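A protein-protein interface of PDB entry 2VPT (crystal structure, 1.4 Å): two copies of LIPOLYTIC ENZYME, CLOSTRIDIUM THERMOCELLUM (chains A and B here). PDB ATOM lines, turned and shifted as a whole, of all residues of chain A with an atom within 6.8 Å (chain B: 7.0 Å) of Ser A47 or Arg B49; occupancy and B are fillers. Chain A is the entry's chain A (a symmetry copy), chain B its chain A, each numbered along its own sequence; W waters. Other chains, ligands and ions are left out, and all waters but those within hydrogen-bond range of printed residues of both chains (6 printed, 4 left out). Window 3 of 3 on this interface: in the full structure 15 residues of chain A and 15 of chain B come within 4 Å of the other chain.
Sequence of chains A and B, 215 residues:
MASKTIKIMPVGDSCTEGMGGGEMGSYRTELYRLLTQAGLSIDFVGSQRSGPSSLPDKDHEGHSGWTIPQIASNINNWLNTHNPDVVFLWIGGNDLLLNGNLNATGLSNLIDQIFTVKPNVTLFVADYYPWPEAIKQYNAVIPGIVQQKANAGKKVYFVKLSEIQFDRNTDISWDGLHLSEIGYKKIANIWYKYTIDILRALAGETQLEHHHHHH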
ATOM      1  N   MET A   9      -9.195 -32.665  11.204  1.00  0.00           N
ATOM      2  CA  MET A   9      -9.276 -31.399  11.914  1.00  0.00           C
ATOM      3  C   MET A   9     -10.709 -30.884  11.905  1.00  0.00           C
ATOM      4  O   MET A   9     -11.203 -30.431  10.865  1.00  0.00           O
ATOM      5  CB  MET A   9      -8.371 -30.361  11.277  1.00  0.00           C
ATOM      6  CG  MET A   9      -8.313 -29.074  12.099  1.00  0.00           C
ATOM      7  SD  MET A   9      -7.250 -27.707  11.282  1.00  0.00           S
ATOM      8  CE  MET A   9      -6.241 -28.158  11.691  1.00  0.00           C
ATOM      9  N   GLU A  17     -16.795 -26.478  19.002  1.00  0.00           N
ATOM     10  CA  GLU A  17     -16.191 -26.420  20.327  1.00  0.00           C
ATOM     11  C   GLU A  17     -17.061 -27.157  21.339  1.00  0.00           C
ATOM     12  O   GLU A  17     -16.535 -27.822  22.239  1.00  0.00           O
ATOM     13  CB  GLU A  17     -15.910 -24.980  20.755  1.00  0.00           C
ATOM     14  CG  GLU A  17     -15.088 -24.884  22.045  1.00  0.00           C
ATOM     15  CD  GLU A  17     -14.427 -23.532  22.247  1.00  0.00           C
ATOM     16  OE1 GLU A  17     -14.968 -22.505  21.777  1.00  0.00           O
ATOM     17  OE2 GLU A  17     -13.365 -23.523  22.893  1.00  0.00           O
ATOM     18  N   VAL A  45      -7.134 -33.559  15.257  1.00  0.00           N
ATOM     19  CA  VAL A  45      -6.069 -32.601  15.415  1.00  0.00           C
ATOM     20  C   VAL A  45      -6.569 -31.162  15.488  1.00  0.00           C
ATOM     21  O   VAL A  45      -7.614 -30.812  14.941  1.00  0.00           O
ATOM     22  CB  VAL A  45      -5.000 -32.764  14.286  1.00  0.00           C
ATOM     23  CG1 VAL A  45      -4.382 -34.166  14.309  1.00  0.00           C
ATOM     24  CG2 VAL A  45      -5.578 -32.449  12.902  1.00  0.00           C
ATOM     25  N   GLY A  46      -5.782 -30.329  16.145  1.00  0.00           N
ATOM     26  CA  GLY A  46      -6.120 -28.929  16.372  1.00  0.00           C
ATOM     27  C   GLY A  46      -5.525 -28.466  17.685  1.00  0.00           C
ATOM     28  O   GLY A  46      -5.137 -29.297  18.515  1.00  0.00           O
ATOM     29  N   SER A  47      -5.403 -27.162  17.891  1.00  0.00           N
ATOM     30  CA  SER A  47      -4.756 -26.693  19.112  1.00  0.00           C
ATOM     31  C   SER A  47      -5.710 -26.562  20.295  1.00  0.00           C
ATOM     32  O   SER A  47      -5.265 -26.616  21.450  1.00  0.00           O
ATOM     33  CB  SER A  47      -3.964 -25.404  18.890  1.00  0.00           C
ATOM     34  OG  SER A  47      -2.902 -25.646  17.981  1.00  0.00           O
ATOM     35  N   GLN A  48      -7.018 -26.434  20.040  1.00  0.00           N
ATOM     36  CA  GLN A  48      -7.986 -26.391  21.145  1.00  0.00           C
ATOM     37  C   GLN A  48      -8.043 -27.768  21.778  1.00  0.00           C
ATOM     38  O   GLN A  48      -7.712 -28.758  21.131  1.00  0.00           O
ATOM     39  CB  GLN A  48      -9.383 -26.065  20.641  1.00  0.00           C
ATOM     40  CG  GLN A  48      -9.515 -24.753  19.869  1.00  0.00           C
ATOM     41  CD  GLN A  48      -9.635 -23.570  20.760  1.00  0.00           C
ATOM     42  OE1 GLN A  48      -8.658 -23.157  21.399  1.00  0.00           O
ATOM     43  NE2 GLN A  48     -10.834 -23.010  20.830  1.00  0.00           N
ATOM     44  N   ARG A  49      -8.442 -27.847  23.042  1.00  0.00           N
ATOM     45  CA  ARG A  49      -8.644 -29.156  23.672  1.00  0.00           C
ATOM     46  C   ARG A  49      -9.766 -29.053  24.689  1.00  0.00           C
ATOM     47  O   ARG A  49      -9.695 -28.288  25.651  1.00  0.00           O
ATOM     48  CB  ARG A  49      -7.336 -29.703  24.274  1.00  0.00           C
ATOM     49  CG  ARG A  49      -7.436 -31.118  24.871  1.00  0.00           C
ATOM     50  CD  ARG A  49      -6.215 -32.070  24.613  1.00  0.00           C
ATOM     51  NE  ARG A  49      -4.909 -31.436  24.441  1.00  0.00           N
ATOM     52  CZ  ARG A  49      -3.844 -31.974  23.828  1.00  0.00           C
ATOM     53  NH1 ARG A  49      -3.886 -33.179  23.269  1.00  0.00           N
ATOM     54  NH2 ARG A  49      -2.715 -31.282  23.750  1.00  0.00           N
ATOM     55  N   SER A  50     -10.823 -29.822  24.443  1.00  0.00           N
ATOM     56  CA  SER A  50     -11.974 -29.837  25.323  1.00  0.00           C
ATOM     57  C   SER A  50     -12.802 -31.080  25.090  1.00  0.00           C
ATOM     58  O   SER A  50     -12.809 -31.632  23.990  1.00  0.00           O
ATOM     59  CB  SER A  50     -12.854 -28.604  25.120  1.00  0.00           C
ATOM     60  OG  SER A  50     -13.494 -28.569  23.855  1.00  0.00           O
ATOM     61  N   ASP A  59      -8.706 -32.993  20.906  1.00  0.00           N
ATOM     62  CA  ASP A  59      -8.149 -31.911  20.095  1.00  0.00           C
ATOM     63  C   ASP A  59      -9.116 -31.450  19.017  1.00  0.00           C
ATOM     64  O   ASP A  59      -9.824 -32.258  18.422  1.00  0.00           O
ATOM     65  CB  ASP A  59      -6.855 -32.360  19.429  1.00  0.00           C
ATOM     66  CG  ASP A  59      -5.864 -32.926  20.418  1.00  0.00           C
ATOM     67  OD1 ASP A  59      -5.624 -32.299  21.473  1.00  0.00           O
ATOM     68  OD2 ASP A  59      -5.335 -34.024  20.140  1.00  0.00           O
ATOM     69  N   HIS A  60      -9.136 -30.148  18.751  1.00  0.00           N
ATOM     70  CA  HIS A  60     -10.021 -29.618  17.705  1.00  0.00           C
ATOM     71  C   HIS A  60      -9.660 -28.174  17.358  1.00  0.00           C
ATOM     72  O   HIS A  60      -8.782 -27.576  17.982  1.00  0.00           O
ATOM     73  CB  HIS A  60     -11.487 -29.706  18.128  1.00  0.00           C
ATOM     74  CG  HIS A  60     -11.837 -28.879  19.324  1.00  0.00           C
ATOM     75  ND1 HIS A  60     -12.185 -27.545  19.235  1.00  0.00           N
ATOM     76  CD2 HIS A  60     -11.898 -29.195  20.640  1.00  0.00           C
ATOM     77  CE1 HIS A  60     -12.452 -27.082  20.447  1.00  0.00           C
ATOM     78  NE2 HIS A  60     -12.287 -28.067  21.319  1.00  0.00           N
ATOM     79  N   GLU A  61     -10.351 -27.622  16.354  1.00  0.00           N
ATOM     80  CA  GLU A  61     -10.256 -26.186  16.009  1.00  0.00           C
ATOM     81  C   GLU A  61     -11.652 -25.564  15.926  1.00  0.00           C
ATOM     82  O   GLU A  61     -11.990 -24.841  14.971  1.00  0.00           O
ATOM     83  CB  GLU A  61      -9.494 -25.940  14.705  1.00  0.00           C
ATOM     84  CG  GLU A  61      -8.002 -26.089  14.781  1.00  0.00           C
ATOM     85  CD  GLU A  61      -7.254 -25.103  15.653  1.00  0.00           C
ATOM     86  OE1 GLU A  61      -7.781 -24.098  16.214  1.00  0.00           O
ATOM     87  OE2 GLU A  61      -6.075 -25.398  15.869  1.00  0.00           O
ATOM     88  N   HIS A  63     -14.089 -22.835  17.568  1.00  0.00           N
ATOM     89  CA  HIS A  63     -13.947 -21.554  18.247  1.00  0.00           C
ATOM     90  C   HIS A  63     -15.298 -20.883  18.423  1.00  0.00           C
ATOM     91  O   HIS A  63     -15.849 -20.318  17.476  1.00  0.00           O
ATOM     92  CB  HIS A  63     -13.022 -20.652  17.423  1.00  0.00           C
ATOM     93  CG  HIS A  63     -11.609 -21.125  17.407  1.00  0.00           C
ATOM     94  ND1 HIS A  63     -11.121 -22.089  16.543  1.00  0.00           N
ATOM     95  CD2 HIS A  63     -10.584 -20.809  18.227  1.00  0.00           C
ATOM     96  CE1 HIS A  63      -9.856 -22.332  16.847  1.00  0.00           C
ATOM     97  NE2 HIS A  63      -9.501 -21.538  17.835  1.00  0.00           N
ATOM     98  N   TRP A  78      -3.227 -23.094  11.008  1.00  0.00           N
ATOM     99  CA  TRP A  78      -3.711 -24.336  11.600  1.00  0.00           C
ATOM    100  C   TRP A  78      -3.418 -25.520  10.677  1.00  0.00           C
ATOM    101  O   TRP A  78      -2.976 -26.574  11.122  1.00  0.00           O
ATOM    102  CB  TRP A  78      -5.214 -24.250  11.857  1.00  0.00           C
ATOM    103  CG  TRP A  78      -5.632 -23.135  12.757  1.00  0.00           C
ATOM    104  CD1 TRP A  78      -4.853 -22.430  13.630  1.00  0.00           C
ATOM    105  CD2 TRP A  78      -6.948 -22.624  12.901  1.00  0.00           C
ATOM    106  NE1 TRP A  78      -5.602 -21.490  14.275  1.00  0.00           N
ATOM    107  CE2 TRP A  78      -6.902 -21.606  13.868  1.00  0.00           C
ATOM    108  CE3 TRP A  78      -8.171 -22.947  12.320  1.00  0.00           C
ATOM    109  CZ2 TRP A  78      -8.029 -20.884  14.247  1.00  0.00           C
ATOM    110  CZ3 TRP A  78      -9.289 -22.224  12.699  1.00  0.00           C
ATOM    111  CH2 TRP A  78      -9.208 -21.212  13.648  1.00  0.00           C
ATOM    112  N   THR A  81       0.326 -26.237  10.725  1.00  0.00           N
ATOM    113  CA  THR A  81       0.740 -26.782  12.008  1.00  0.00           C
ATOM    114  C   THR A  81       0.321 -28.239  12.175  1.00  0.00           C
ATOM    115  O   THR A  81       1.113 -29.077  12.608  1.00  0.00           O
ATOM    116  CB  THR A  81       0.160 -25.952  13.164  1.00  0.00           C
ATOM    117  OG1 THR A  81       0.719 -24.631  13.127  1.00  0.00           O
ATOM    118  CG2 THR A  81       0.465 -26.587  14.516  1.00  0.00           C
ATOM    119  N   HIS A  82      -0.914 -28.555  11.798  1.00  0.00           N
ATOM    120  CA  HIS A  82      -1.488 -29.872  12.112  1.00  0.00           C
ATOM    121  C   HIS A  82      -1.525 -30.842  10.939  1.00  0.00           C
ATOM    122  O   HIS A  82      -1.689 -32.042  11.147  1.00  0.00           O
ATOM    123  CB  HIS A  82      -2.879 -29.697  12.718  1.00  0.00           C
ATOM    124  CG  HIS A  82      -2.861 -28.921  13.992  1.00  0.00           C
ATOM    125  ND1 HIS A  82      -2.316 -29.422  15.155  1.00  0.00           N
ATOM    126  CD2 HIS A  82      -3.270 -27.663  14.275  1.00  0.00           C
ATOM    127  CE1 HIS A  82      -2.413 -28.510  16.105  1.00  0.00           C
ATOM    128  NE2 HIS A  82      -2.979 -27.430  15.597  1.00  0.00           N
ATOM    129  N   GLU B  17     -13.595 -23.024  32.844  1.00  0.00           N
ATOM    130  CA  GLU B  17     -13.512 -23.318  31.418  1.00  0.00           C
ATOM    131  C   GLU B  17     -13.984 -22.121  30.602  1.00  0.00           C
ATOM    132  O   GLU B  17     -13.416 -21.831  29.542  1.00  0.00           O
ATOM    133  CB  GLU B  17     -14.276 -24.592  31.061  1.00  0.00           C
ATOM    134  CG  GLU B  17     -14.042 -25.051  29.617  1.00  0.00           C
ATOM    135  CD  GLU B  17     -14.409 -26.502  29.372  1.00  0.00           C
ATOM    136  OE1 GLU B  17     -15.316 -27.034  30.053  1.00  0.00           O
ATOM    137  OE2 GLU B  17     -13.776 -27.094  28.479  1.00  0.00           O
ATOM    138  N   MET B  24     -14.664 -18.706  25.826  1.00  0.00           N
ATOM    139  CA  MET B  24     -14.074 -19.770  26.642  1.00  0.00           C
ATOM    140  C   MET B  24     -12.722 -19.387  27.227  1.00  0.00           C
ATOM    141  O   MET B  24     -11.839 -20.219  27.426  1.00  0.00           O
ATOM    142  CB  MET B  24     -14.012 -21.093  25.871  1.00  0.00           C
ATOM    143  CG  MET B  24     -15.296 -21.491  25.160  1.00  0.00           C
ATOM    144  SD  MET B  24     -16.809 -21.924  26.305  1.00  0.00           S
ATOM    145  CE  MET B  24     -15.869 -22.908  27.278  1.00  0.00           C
ATOM    146  N   ARG B  28      -9.433 -15.951  32.818  1.00  0.00           N
ATOM    147  CA  ARG B  28      -8.024 -16.150  32.463  1.00  0.00           C
ATOM    148  C   ARG B  28      -7.524 -15.081  31.491  1.00  0.00           C
ATOM    149  O   ARG B  28      -6.386 -14.630  31.598  1.00  0.00           O
ATOM    150  CB  ARG B  28      -7.803 -17.565  31.918  1.00  0.00           C
ATOM    151  CG  ARG B  28      -8.003 -18.632  33.010  1.00  0.00           C
ATOM    152  CD  ARG B  28      -8.073 -20.038  32.481  1.00  0.00           C
ATOM    153  NE  ARG B  28      -9.318 -20.349  31.786  1.00  0.00           N
ATOM    154  CZ  ARG B  28      -9.478 -20.460  30.465  1.00  0.00           C
ATOM    155  NH1 ARG B  28      -8.498 -20.232  29.595  1.00  0.00           N
ATOM    156  NH2 ARG B  28     -10.671 -20.762  30.006  1.00  0.00           N
ATOM    157  N   PHE B  44       0.151 -20.393  32.625  1.00  0.00           N
ATOM    158  CA  PHE B  44      -1.035 -21.161  32.971  1.00  0.00           C
ATOM    159  C   PHE B  44      -0.806 -22.580  32.497  1.00  0.00           C
ATOM    160  O   PHE B  44      -0.385 -22.800  31.361  1.00  0.00           O
ATOM    161  CB  PHE B  44      -2.297 -20.590  32.324  1.00  0.00           C
ATOM    162  CG  PHE B  44      -2.895 -19.388  33.028  1.00  0.00           C
ATOM    163  CD1 PHE B  44      -3.000 -19.329  34.413  1.00  0.00           C
ATOM    164  CD2 PHE B  44      -3.451 -18.346  32.291  1.00  0.00           C
ATOM    165  CE1 PHE B  44      -3.590 -18.237  35.023  1.00  0.00           C
ATOM    166  CE2 PHE B  44      -4.063 -17.268  32.909  1.00  0.00           C
ATOM    167  CZ  PHE B  44      -4.123 -17.204  34.274  1.00  0.00           C
ATOM    168  N   GLY B  46      -2.217 -26.856  32.439  1.00  0.00           N
ATOM    169  CA  GLY B  46      -3.375 -27.743  32.430  1.00  0.00           C
ATOM    170  C   GLY B  46      -3.540 -28.353  31.054  1.00  0.00           C
ATOM    171  O   GLY B  46      -2.957 -27.856  30.084  1.00  0.00           O
ATOM    172  N   SER B  47      -4.285 -29.444  30.939  1.00  0.00           N
ATOM    173  CA  SER B  47      -4.391 -30.098  29.639  1.00  0.00           C
ATOM    174  C   SER B  47      -5.494 -29.523  28.756  1.00  0.00           C
ATOM    175  O   SER B  47      -5.421 -29.648  27.527  1.00  0.00           O
ATOM    176  CB  SER B  47      -4.512 -31.618  29.764  1.00  0.00           C
ATOM    177  OG  SER B  47      -3.331 -32.146  30.346  1.00  0.00           O
ATOM    178  N   GLN B  48      -6.494 -28.860  29.348  1.00  0.00           N
ATOM    179  CA  GLN B  48      -7.535 -28.213  28.535  1.00  0.00           C
ATOM    180  C   GLN B  48      -6.910 -27.031  27.819  1.00  0.00           C
ATOM    181  O   GLN B  48      -5.898 -26.503  28.271  1.00  0.00           O
ATOM    182  CB  GLN B  48      -8.659 -27.675  29.407  1.00  0.00           C
ATOM    183  CG  GLN B  48      -9.352 -28.704  30.299  1.00  0.00           C
ATOM    184  CD  GLN B  48     -10.384 -29.492  29.575  1.00  0.00           C
ATOM    185  OE1 GLN B  48     -10.057 -30.352  28.746  1.00  0.00           O
ATOM    186  NE2 GLN B  48     -11.645 -29.207  29.863  1.00  0.00           N
ATOM    187  N   ARG B  49      -7.487 -26.617  26.698  1.00  0.00           N
ATOM    188  CA  ARG B  49      -7.013 -25.402  26.027  1.00  0.00           C
ATOM    189  C   ARG B  49      -8.183 -24.719  25.345  1.00  0.00           C
ATOM    190  O   ARG B  49      -8.837 -25.284  24.468  1.00  0.00           O
ATOM    191  CB  ARG B  49      -5.849 -25.703  25.066  1.00  0.00           C
ATOM    192  CG  ARG B  49      -5.224 -24.468  24.393  1.00  0.00           C
ATOM    193  CD  ARG B  49      -3.662 -24.471  24.245  1.00  0.00           C
ATOM    194  NE  ARG B  49      -3.012 -25.777  24.132  1.00  0.00           N
ATOM    195  CZ  ARG B  49      -1.726 -26.046  24.402  1.00  0.00           C
ATOM    196  NH1 ARG B  49      -0.889 -25.113  24.846  1.00  0.00           N
ATOM    197  NH2 ARG B  49      -1.269 -27.281  24.250  1.00  0.00           N
ATOM    198  N   SER B  50      -8.457 -23.493  25.784  1.00  0.00           N
ATOM    199  CA  SER B  50      -9.542 -22.710  25.230  1.00  0.00           C
ATOM    200  C   SER B  50      -9.359 -21.246  25.557  1.00  0.00           C
ATOM    201  O   SER B  50      -8.750 -20.900  26.570  1.00  0.00           O
ATOM    202  CB  SER B  50     -10.899 -23.176  25.759  1.00  0.00           C
ATOM    203  OG  SER B  50     -11.080 -22.929  27.143  1.00  0.00           O
ATOM    204  N   GLY B  51      -9.928 -20.391  24.720  1.00  0.00           N
ATOM    205  CA  GLY B  51      -9.861 -18.977  24.951  1.00  0.00           C
ATOM    206  C   GLY B  51      -9.954 -18.200  23.662  1.00  0.00           C
ATOM    207  O   GLY B  51      -9.843 -18.771  22.581  1.00  0.00           O
ATOM    208  N   PRO B  56      -2.757 -15.198  25.254  1.00  0.00           N
ATOM    209  CA  PRO B  56      -1.614 -15.962  24.748  1.00  0.00           C
ATOM    210  C   PRO B  56      -1.483 -17.380  25.297  1.00  0.00           C
ATOM    211  O   PRO B  56      -0.994 -18.265  24.615  1.00  0.00           O
ATOM    212  CB  PRO B  56      -0.406 -15.079  25.144  1.00  0.00           C
ATOM    213  CG  PRO B  56      -0.988 -13.731  25.337  1.00  0.00           C
ATOM    214  CD  PRO B  56      -2.314 -13.989  25.973  1.00  0.00           C
ATOM    215  N   ASP B  57      -1.931 -17.571  26.527  1.00  0.00           N
ATOM    216  CA  ASP B  57      -1.757 -18.833  27.227  1.00  0.00           C
ATOM    217  C   ASP B  57      -3.129 -19.359  27.639  1.00  0.00           C
ATOM    218  O   ASP B  57      -3.745 -18.880  28.604  1.00  0.00           O
ATOM    219  CB  ASP B  57      -0.850 -18.648  28.445  1.00  0.00           C
ATOM    220  CG  ASP B  57      -0.395 -19.964  29.032  1.00  0.00           C
ATOM    221  OD1 ASP B  57      -1.087 -20.983  28.789  1.00  0.00           O
ATOM    222  OD2 ASP B  57       0.651 -20.002  29.741  1.00  0.00           O
ATOM    223  N   LYS B  58      -3.602 -20.335  26.867  1.00  0.00           N
ATOM    224  CA  LYS B  58      -4.981 -20.806  26.943  1.00  0.00           C
ATOM    225  C   LYS B  58      -5.116 -22.122  27.723  1.00  0.00           C
ATOM    226  O   LYS B  58      -6.204 -22.721  27.759  1.00  0.00           O
ATOM    227  CB  LYS B  58      -5.536 -20.982  25.527  1.00  0.00           C
ATOM    228  CG  LYS B  58      -5.573 -19.690  24.707  1.00  0.00           C
ATOM    229  CD  LYS B  58      -5.863 -19.965  23.206  1.00  0.00           C
ATOM    230  CE  LYS B  58      -5.621 -18.741  22.283  1.00  0.00           C
ATOM    231  NZ  LYS B  58      -4.194 -18.402  22.144  1.00  0.00           N
ATOM    232  N   ASP B  59      -4.040 -22.564  28.371  1.00  0.00           N
ATOM    233  CA  ASP B  59      -4.063 -23.829  29.103  1.00  0.00           C
ATOM    234  C   ASP B  59      -4.796 -23.706  30.429  1.00  0.00           C
ATOM    235  O   ASP B  59      -4.693 -22.691  31.112  1.00  0.00           O
ATOM    236  CB  ASP B  59      -2.644 -24.310  29.374  1.00  0.00           C
ATOM    237  CG  ASP B  59      -1.808 -24.371  28.119  1.00  0.00           C
ATOM    238  OD1 ASP B  59      -2.274 -24.922  27.097  1.00  0.00           O
ATOM    239  OD2 ASP B  59      -0.675 -23.844  28.155  1.00  0.00           O
ATOM    240  N   HIS B  60      -5.528 -24.750  30.804  1.00  0.00           N
ATOM    241  CA  HIS B  60      -6.250 -24.730  32.085  1.00  0.00           C
ATOM    242  C   HIS B  60      -6.757 -26.123  32.453  1.00  0.00           C
ATOM    243  O   HIS B  60      -6.614 -27.071  31.680  1.00  0.00           O
ATOM    244  CB  HIS B  60      -7.413 -23.739  32.044  1.00  0.00           C
ATOM    245  CG  HIS B  60      -8.481 -24.079  31.055  1.00  0.00           C
ATOM    246  ND1 HIS B  60      -9.526 -24.936  31.347  1.00  0.00           N
ATOM    247  CD2 HIS B  60      -8.674 -23.675  29.775  1.00  0.00           C
ATOM    248  CE1 HIS B  60     -10.316 -25.036  30.289  1.00  0.00           C
ATOM    249  NE2 HIS B  60      -9.821 -24.277  29.321  1.00  0.00           N
ATOM    250  N   GLU B  61      -7.356 -26.232  33.644  1.00  0.00           N
ATOM    251  CA  GLU B  61      -8.062 -27.460  34.078  1.00  0.00           C
ATOM    252  C   GLU B  61      -9.470 -27.119  34.569  1.00  0.00           C
ATOM    253  O   GLU B  61      -9.917 -27.572  35.640  1.00  0.00           O
ATOM    254  CB  GLU B  61      -7.299 -28.228  35.160  1.00  0.00           C
ATOM    255  CG  GLU B  61      -6.101 -29.002  34.693  1.00  0.00           C
ATOM    256  CD  GLU B  61      -6.354 -30.158  33.748  1.00  0.00           C
ATOM    257  OE1 GLU B  61      -7.501 -30.589  33.431  1.00  0.00           O
ATOM    258  OE2 GLU B  61      -5.339 -30.616  33.213  1.00  0.00           O
HETATM  259  O   HOH W   1     -11.642 -25.747  23.404  1.00  0.00           O
HETATM  260  O   HOH W   2     -11.265 -26.324  27.352  1.00  0.00           O
HETATM  261  O   HOH W   3      -3.394 -31.267  26.767  1.00  0.00           O
HETATM  262  O   HOH W   4      -2.563 -26.619  21.520  1.00  0.00           O
HETATM  263  O   HOH W   5      -8.439 -20.443  20.947  1.00  0.00           O
HETATM  264  O   HOH W   6     -11.958 -21.236  22.838  1.00  0.00           O
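O of Arg B49 sits at hydrogen-bond distance from N of Arg A49 (3.0 Å).
The guanidinium group (NH2) of Arg B28 sits at hydrogen-bond distance from the backbone carbonyl oxygen (O) of Met B24. The backbone NH (N) of Gln B48 lies within hydrogen-bond range of the backbone carbonyl oxygen (O) of His B60 (2.9 Å). NH1 of Arg B49 is in salt-bridge range of OD1 of Asp B59. A ring nitrogen (NE2) of His A82 is in hydrogen-bond range of the side-chain hydroxyl (OG) of Ser A47, at 3.0 Å. NH1 of Arg A49 is in salt-bridge range of OD1 of Asp A59 (2.6 Å). NE2 of His A60 lies within hydrogen-bond range of OG of Ser A50, 2.9 Å away.
Among the printed residues, pairs that only touch across the chains: Glu A17 with Met B24, Ser A47 with Arg B49, Arg A49 with Ser B47, Arg A49 with Gln B48, Gln A48 with Arg B49, Ser A50 with Glu B17, Glu A17 with Ser B50, Ser A50 with Gln B48 and Gln A48 with Ser B50.
Printed residues of chain B within 4 Å of Ser A47: Arg B49. Printed residues of chain A within 4 Å of Arg B49: Ser A47, Gln A48 and Arg A49. Printed residues of chain B within 4 Å of Glu A17: Met B24 (3.5 Å) and Ser B50 (3.8 Å). Of the printed residues of chain B, Arg A49 touches Ser B47, Gln B48 and Arg B49. Of the printed residues of chain A, Ser B50 touches Glu A17 and Gln A48. Of the printed residues of chain B, Gln A48 touches Arg B49 (3.6 Å) and Ser B50 (3.96 Å). Phe B44 touches none of the printed residues of chain A. His A82 touches none of the printed residues of chain B.
Hydrophobic or aromatic side chains of chain B within 4 Å of the printed part of chain A: Met B24. Printed residues of chain A that touch a printed residue of chain B: Glu A17, Ser A47, Gln A48, Arg A49 and Ser A50. Among the printed residues, no Asp or Glu carboxylate lies within 4 Å of a Lys or Arg side-chain nitrogen of the other chain.
Glu A17 touches Ser B50, and with the chains exchanged Ser A50 touches Glu B17. Gln A48 touches Arg B49, and with the chains exchanged Arg A49 touches Gln B48. Gln A48 touches Ser B50, and with the chains exchanged Ser A50 touches Gln B48. Arg A49 touches its own counterpart, Arg B49. Of the 10 pairs that touch across the chains among the printed residues, 9 have their exchanged pair printed and touching as well.
Water W6 lies within hydrogen-bond range of the side-chain carboxylate of Glu A17 (2.7 Å), the backbone NH of Gly B51 (2.9 Å) and the side-chain amide nitrogen of Gln A48 (2.9 Å). Water W4 bridges O of Ser A47 (2.7 Å) and NE of Arg B49 (2.8 Å). Water W3 lies within hydrogen-bond range of O of Ser B47 (2.7 Å) and NE of Arg A49 (2.8 Å). Water W5 lies within hydrogen-bond range of O of Gly B51 (2.7 Å), OE1 of Gln A48 (2.8 Å) and NE2 of His A63 (3.5 Å). Water W2 lies within hydrogen-bond range of the side-chain carboxylate of Glu B17 (2.9 Å), the backbone carbonyl oxygen of Arg A49 (3.0 Å), a ring nitrogen (NE2) of His B60 (3.2 Å) and the side-chain hydroxyl of Ser B50 (3.4 Å). Water W1 lies within hydrogen-bond range of the side-chain carboxylate of Glu A17 (2.9 Å), the backbone carbonyl oxygen of Arg B49 (3.0 Å), a ring nitrogen (NE2) of His A60 (3.2 Å) and the side-chain hydroxyl of Ser A50 (3.4 Å).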
